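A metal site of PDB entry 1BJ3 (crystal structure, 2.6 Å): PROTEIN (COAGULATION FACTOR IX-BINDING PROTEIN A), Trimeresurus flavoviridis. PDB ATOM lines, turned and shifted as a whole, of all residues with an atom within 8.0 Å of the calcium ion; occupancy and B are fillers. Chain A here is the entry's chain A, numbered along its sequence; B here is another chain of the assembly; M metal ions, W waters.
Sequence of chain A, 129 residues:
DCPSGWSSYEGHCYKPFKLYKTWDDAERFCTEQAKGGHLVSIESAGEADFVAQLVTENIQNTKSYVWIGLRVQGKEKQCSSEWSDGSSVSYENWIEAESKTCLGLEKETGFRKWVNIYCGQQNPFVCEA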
ATOM      1  N   TYR A   9      -3.078 -16.242   8.610  1.00  0.00           N
ATOM      2  CA  TYR A   9      -2.564 -15.746   9.865  1.00  0.00           C
ATOM      3  C   TYR A   9      -2.546 -14.230   9.780  1.00  0.00           C
ATOM      4  O   TYR A   9      -1.908 -13.638   8.914  1.00  0.00           O
ATOM      5  CB  TYR A   9      -1.175 -16.295  10.173  1.00  0.00           C
ATOM      6  CG  TYR A   9      -0.579 -15.677  11.427  1.00  0.00           C
ATOM      7  CD1 TYR A   9      -0.990 -16.093  12.689  1.00  0.00           C
ATOM      8  CD2 TYR A   9       0.370 -14.665  11.346  1.00  0.00           C
ATOM      9  CE1 TYR A   9      -0.467 -15.501  13.841  1.00  0.00           C
ATOM     10  CE2 TYR A   9       0.885 -14.071  12.466  1.00  0.00           C
ATOM     11  CZ  TYR A   9       0.471 -14.495  13.716  1.00  0.00           C
ATOM     12  OH  TYR A   9       1.007 -13.893  14.835  1.00  0.00           O
ATOM     13  N   GLU A  10      -3.347 -13.615  10.638  1.00  0.00           N
ATOM     14  CA  GLU A  10      -3.486 -12.174  10.719  1.00  0.00           C
ATOM     15  C   GLU A  10      -3.667 -11.457   9.377  1.00  0.00           C
ATOM     16  O   GLU A  10      -2.895 -10.579   9.023  1.00  0.00           O
ATOM     17  CB  GLU A  10      -2.332 -11.558  11.531  1.00  0.00           C
ATOM     18  CG  GLU A  10      -2.170 -12.185  12.891  1.00  0.00           C
ATOM     19  CD  GLU A  10      -1.598 -11.243  13.924  1.00  0.00           C
ATOM     20  OE1 GLU A  10      -0.508 -10.633  13.697  1.00  0.00           O
ATOM     21  OE2 GLU A  10      -2.222 -11.114  14.996  1.00  0.00           O
ATOM     22  N   HIS A  12      -3.390 -12.450   6.072  1.00  0.00           N
ATOM     23  CA  HIS A  12      -2.342 -12.630   5.090  1.00  0.00           C
ATOM     24  C   HIS A  12      -2.448 -14.095   4.720  1.00  0.00           C
ATOM     25  O   HIS A  12      -3.007 -14.881   5.489  1.00  0.00           O
ATOM     26  CB  HIS A  12      -0.996 -12.337   5.747  1.00  0.00           C
ATOM     27  CG  HIS A  12      -0.362 -11.069   5.294  1.00  0.00           C
ATOM     28  ND1 HIS A  12      -0.921  -9.834   5.522  1.00  0.00           N
ATOM     29  CD2 HIS A  12       0.798 -10.838   4.637  1.00  0.00           C
ATOM     30  CE1 HIS A  12      -0.121  -8.889   5.046  1.00  0.00           C
ATOM     31  NE2 HIS A  12       0.933  -9.481   4.510  1.00  0.00           N
ATOM     32  N   TYR A  14      -0.446 -17.605   3.336  1.00  0.00           N
ATOM     33  CA  TYR A  14       0.858 -18.192   3.208  1.00  0.00           C
ATOM     34  C   TYR A  14       0.838 -19.536   2.519  1.00  0.00           C
ATOM     35  O   TYR A  14      -0.025 -20.372   2.811  1.00  0.00           O
ATOM     36  CB  TYR A  14       1.473 -18.332   4.616  1.00  0.00           C
ATOM     37  CG  TYR A  14       1.626 -17.020   5.377  1.00  0.00           C
ATOM     38  CD1 TYR A  14       0.528 -16.424   5.997  1.00  0.00           C
ATOM     39  CD2 TYR A  14       2.865 -16.406   5.482  1.00  0.00           C
ATOM     40  CE1 TYR A  14       0.658 -15.227   6.714  1.00  0.00           C
ATOM     41  CE2 TYR A  14       3.016 -15.200   6.197  1.00  0.00           C
ATOM     42  CZ  TYR A  14       1.910 -14.631   6.818  1.00  0.00           C
ATOM     43  OH  TYR A  14       2.051 -13.480   7.569  1.00  0.00           O
ATOM     44  N   LEU A  39       8.084 -13.460  -1.035  1.00  0.00           N
ATOM     45  CA  LEU A  39       8.587 -14.505  -0.162  1.00  0.00           C
ATOM     46  C   LEU A  39       8.161 -14.055   1.217  1.00  0.00           C
ATOM     47  O   LEU A  39       8.134 -12.850   1.471  1.00  0.00           O
ATOM     48  CB  LEU A  39      10.100 -14.555  -0.240  1.00  0.00           C
ATOM     49  CG  LEU A  39      10.655 -15.615  -1.177  1.00  0.00           C
ATOM     50  CD1 LEU A  39      11.971 -15.141  -1.764  1.00  0.00           C
ATOM     51  CD2 LEU A  39      10.791 -16.933  -0.423  1.00  0.00           C
ATOM     52  N   VAL A  40       7.834 -14.963   2.105  1.00  0.00           N
ATOM     53  CA  VAL A  40       7.380 -14.572   3.441  1.00  0.00           C
ATOM     54  C   VAL A  40       8.297 -13.556   4.155  1.00  0.00           C
ATOM     55  O   VAL A  40       9.535 -13.585   4.046  1.00  0.00           O
ATOM     56  CB  VAL A  40       7.114 -15.834   4.341  1.00  0.00           C
ATOM     57  CG1 VAL A  40       8.413 -16.617   4.608  1.00  0.00           C
ATOM     58  CG2 VAL A  40       6.405 -15.454   5.602  1.00  0.00           C
ATOM     59  N   SER A  41       7.672 -12.577   4.812  1.00  0.00           N
ATOM     60  CA  SER A  41       8.362 -11.536   5.574  1.00  0.00           C
ATOM     61  C   SER A  41       8.019 -11.734   7.042  1.00  0.00           C
ATOM     62  O   SER A  41       6.832 -11.598   7.411  1.00  0.00           O
ATOM     63  CB  SER A  41       7.860 -10.173   5.141  1.00  0.00           C
ATOM     64  OG  SER A  41       6.483 -10.037   5.463  1.00  0.00           O
ATOM     65  N   ILE A  42       8.990 -12.123   7.858  1.00  0.00           N
ATOM     66  CA  ILE A  42       8.734 -12.328   9.285  1.00  0.00           C
ATOM     67  C   ILE A  42       9.014 -11.029  10.023  1.00  0.00           C
ATOM     68  O   ILE A  42      10.166 -10.711  10.350  1.00  0.00           O
ATOM     69  CB  ILE A  42       9.529 -13.488   9.905  1.00  0.00           C
ATOM     70  CG1 ILE A  42       9.241 -14.813   9.192  1.00  0.00           C
ATOM     71  CG2 ILE A  42       9.135 -13.633  11.345  1.00  0.00           C
ATOM     72  CD1 ILE A  42       9.920 -14.964   7.860  1.00  0.00           C
ATOM     73  N   GLU A  43       7.941 -10.295  10.286  1.00  0.00           N
ATOM     74  CA  GLU A  43       7.986  -8.992  10.910  1.00  0.00           C
ATOM     75  C   GLU A  43       7.494  -8.956  12.358  1.00  0.00           C
ATOM     76  O   GLU A  43       7.317  -7.881  12.927  1.00  0.00           O
ATOM     77  CB  GLU A  43       7.147  -8.030  10.057  1.00  0.00           C
ATOM     78  CG  GLU A  43       7.529  -8.046   8.582  1.00  0.00           C
ATOM     79  CD  GLU A  43       6.340  -7.733   7.661  1.00  0.00           C
ATOM     80  OE1 GLU A  43       5.331  -8.455   7.794  1.00  0.00           O
ATOM     81  OE2 GLU A  43       6.423  -6.811   6.806  1.00  0.00           O
ATOM     82  N   SER A  44       7.251 -10.128  12.955  1.00  0.00           N
ATOM     83  CA  SER A  44       6.817 -10.203  14.338  1.00  0.00           C
ATOM     84  C   SER A  44       7.143 -11.568  14.940  1.00  0.00           C
ATOM     85  O   SER A  44       7.517 -12.506  14.225  1.00  0.00           O
ATOM     86  CB  SER A  44       5.312  -9.893  14.461  1.00  0.00           C
ATOM     87  OG  SER A  44       4.452 -10.857  13.828  1.00  0.00           O
ATOM     88  N   GLU A  47       4.198 -14.018  14.033  1.00  0.00           N
ATOM     89  CA  GLU A  47       4.333 -14.352  12.629  1.00  0.00           C
ATOM     90  C   GLU A  47       5.408 -15.437  12.373  1.00  0.00           C
ATOM     91  O   GLU A  47       5.184 -16.370  11.588  1.00  0.00           O
ATOM     92  CB  GLU A  47       4.616 -13.100  11.791  1.00  0.00           C
ATOM     93  CG  GLU A  47       5.075 -13.451  10.395  1.00  0.00           C
ATOM     94  CD  GLU A  47       4.869 -12.337   9.402  1.00  0.00           C
ATOM     95  OE1 GLU A  47       5.237 -11.177   9.707  1.00  0.00           O
ATOM     96  OE2 GLU A  47       4.340 -12.620   8.301  1.00  0.00           O
ATOM     97  N   ALA A  48       6.531 -15.329  13.084  1.00  0.00           N
ATOM     98  CA  ALA A  48       7.638 -16.282  12.994  1.00  0.00           C
ATOM     99  C   ALA A  48       7.278 -17.673  13.522  1.00  0.00           C
ATOM    100  O   ALA A  48       7.736 -18.674  12.985  1.00  0.00           O
ATOM    101  CB  ALA A  48       8.807 -15.763  13.751  1.00  0.00           C
ATOM    102  N   VAL A  51       5.071 -19.198  10.830  1.00  0.00           N
ATOM    103  CA  VAL A  51       5.804 -19.627   9.644  1.00  0.00           C
ATOM    104  C   VAL A  51       6.564 -20.910   9.950  1.00  0.00           C
ATOM    105  O   VAL A  51       6.797 -21.699   9.054  1.00  0.00           O
ATOM    106  CB  VAL A  51       6.826 -18.577   9.136  1.00  0.00           C
ATOM    107  CG1 VAL A  51       7.499 -19.072   7.893  1.00  0.00           C
ATOM    108  CG2 VAL A  51       6.159 -17.257   8.869  1.00  0.00           C
ATOM    109  N   GLU A 128       3.976 -15.260   0.594  1.00  0.00           N
ATOM    110  CA  GLU A 128       3.000 -14.576   1.418  1.00  0.00           C
ATOM    111  C   GLU A 128       2.317 -13.476   0.614  1.00  0.00           C
ATOM    112  O   GLU A 128       2.955 -12.714  -0.118  1.00  0.00           O
ATOM    113  CB  GLU A 128       3.700 -14.008   2.636  1.00  0.00           C
ATOM    114  CG  GLU A 128       2.831 -13.198   3.544  1.00  0.00           C
ATOM    115  CD  GLU A 128       3.611 -12.264   4.406  1.00  0.00           C
ATOM    116  OE1 GLU A 128       4.626 -11.723   3.944  1.00  0.00           O
ATOM    117  OE2 GLU A 128       3.211 -12.056   5.554  1.00  0.00           O
ATOM    118  N   ALA A 129       1.007 -13.361   0.806  1.00  0.00           N
ATOM    119  CA  ALA A 129       0.214 -12.385   0.085  1.00  0.00           C
ATOM    120  C   ALA A 129      -0.849 -11.720   0.984  1.00  0.00           C
ATOM    121  O   ALA A 129      -1.493 -12.433   1.780  1.00  0.00           O
ATOM    122  CB  ALA A 129      -0.446 -13.076  -1.110  1.00  0.00           C
ATOM    123  OXT ALA A 129      -0.999 -10.477   0.908  1.00  0.00           O
ATOM    124  N   TRP B  79      13.163  -6.501   3.465  1.00  0.00           N
ATOM    125  CA  TRP B  79      12.405  -7.613   2.930  1.00  0.00           C
ATOM    126  C   TRP B  79      12.006  -7.328   1.502  1.00  0.00           C
ATOM    127  O   TRP B  79      12.053  -6.181   1.059  1.00  0.00           O
ATOM    128  CB  TRP B  79      11.175  -7.841   3.779  1.00  0.00           C
ATOM    129  CG  TRP B  79      11.522  -8.185   5.170  1.00  0.00           C
ATOM    130  CD1 TRP B  79      11.671  -7.306   6.190  1.00  0.00           C
ATOM    131  CD2 TRP B  79      11.750  -9.491   5.718  1.00  0.00           C
ATOM    132  NE1 TRP B  79      11.978  -7.984   7.344  1.00  0.00           N
ATOM    133  CE2 TRP B  79      12.031  -9.331   7.093  1.00  0.00           C
ATOM    134  CE3 TRP B  79      11.740 -10.787   5.182  1.00  0.00           C
ATOM    135  CZ2 TRP B  79      12.302 -10.413   7.942  1.00  0.00           C
ATOM    136  CZ3 TRP B  79      12.012 -11.869   6.031  1.00  0.00           C
ATOM    137  CH2 TRP B  79      12.286 -11.670   7.393  1.00  0.00           C
ATOM    138  N   ASN B  81       9.111  -7.338   0.264  1.00  0.00           N
ATOM    139  CA  ASN B  81       7.863  -6.587   0.155  1.00  0.00           C
ATOM    140  C   ASN B  81       8.134  -5.085   0.397  1.00  0.00           C
ATOM    141  O   ASN B  81       7.210  -4.286   0.535  1.00  0.00           O
ATOM    142  CB  ASN B  81       6.758  -7.128   1.076  1.00  0.00           C
ATOM    143  CG  ASN B  81       7.145  -7.155   2.537  1.00  0.00           C
ATOM    144  OD1 ASN B  81       8.078  -7.827   2.910  1.00  0.00           O
ATOM    145  ND2 ASN B  81       6.398  -6.478   3.353  1.00  0.00           N
ATOM    146  N   ALA B  83       9.624  -3.706   2.951  1.00  0.00           N
ATOM    147  CA  ALA B  83       9.622  -3.340   4.363  1.00  0.00           C
ATOM    148  C   ALA B  83      11.013  -3.209   4.904  1.00  0.00           C
ATOM    149  O   ALA B  83      11.911  -3.981   4.512  1.00  0.00           O
ATOM    150  CB  ALA B  83       8.905  -4.386   5.149  1.00  0.00           C
HETATM  151 CA    CA M   1       4.554 -10.731   7.058  1.00  0.00          CA
HETATM  152  O   HOH W   1       2.701 -10.004   7.939  1.00  0.00           O
HETATM  153  O   HOH W   2       3.796  -8.875   5.535  1.00  0.00           O
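Tyr 14 touches the calcium ion.
Of the 18 residues printed, 5 come within 4 Å of the calcium ion.
The nearest printed residue that does not touch the calcium ion is His 12 (4.5 Å).
Water W2 lies within hydrogen-bond range of a ring nitrogen (NE2) of His 12 (3.1 Å) and the side-chain carboxylate (OE1) of Glu 128 (3.4 Å).
The side-chain hydroxyl (OH) of Tyr 9 is in hydrogen-bond range of the backbone NH (N) of Glu 47 (3.3 Å).
The side-chain hydroxyl of Tyr 14 lies close to the side-chain carboxylate of Glu 128 (2.7 Å).
The backbone NH of Glu 47 sits close to the side-chain hydroxyl of Ser 44 (3.2 Å).
OE2 of Glu 43 lies within hydrogen-bond range of ND2 of Asn 81 of chain B (3.5 Å).
OE2 of Glu 47 sits close to OH of Tyr 14 (2.6 Å).
The calcium ion is bound by water W1 (2.2 Å), the side-chain carboxylate (OE2) of Glu 47 (2.3 Å), the side-chain carboxylate (OE2) of Glu 128 (2.4 Å), the backbone carbonyl oxygen (O) of Ser 41 (2.5 Å), the side-chain carboxylate (OE1) of Glu 43 (2.5 Å), water W2 (2.5 Å), the side-chain hydroxyl (OG) of Ser 41 (2.6 Å) and the side-chain carboxylate (OE1) of Glu 47 (2.8 Å).
The calcium ion has eight donor atoms within binding distance.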
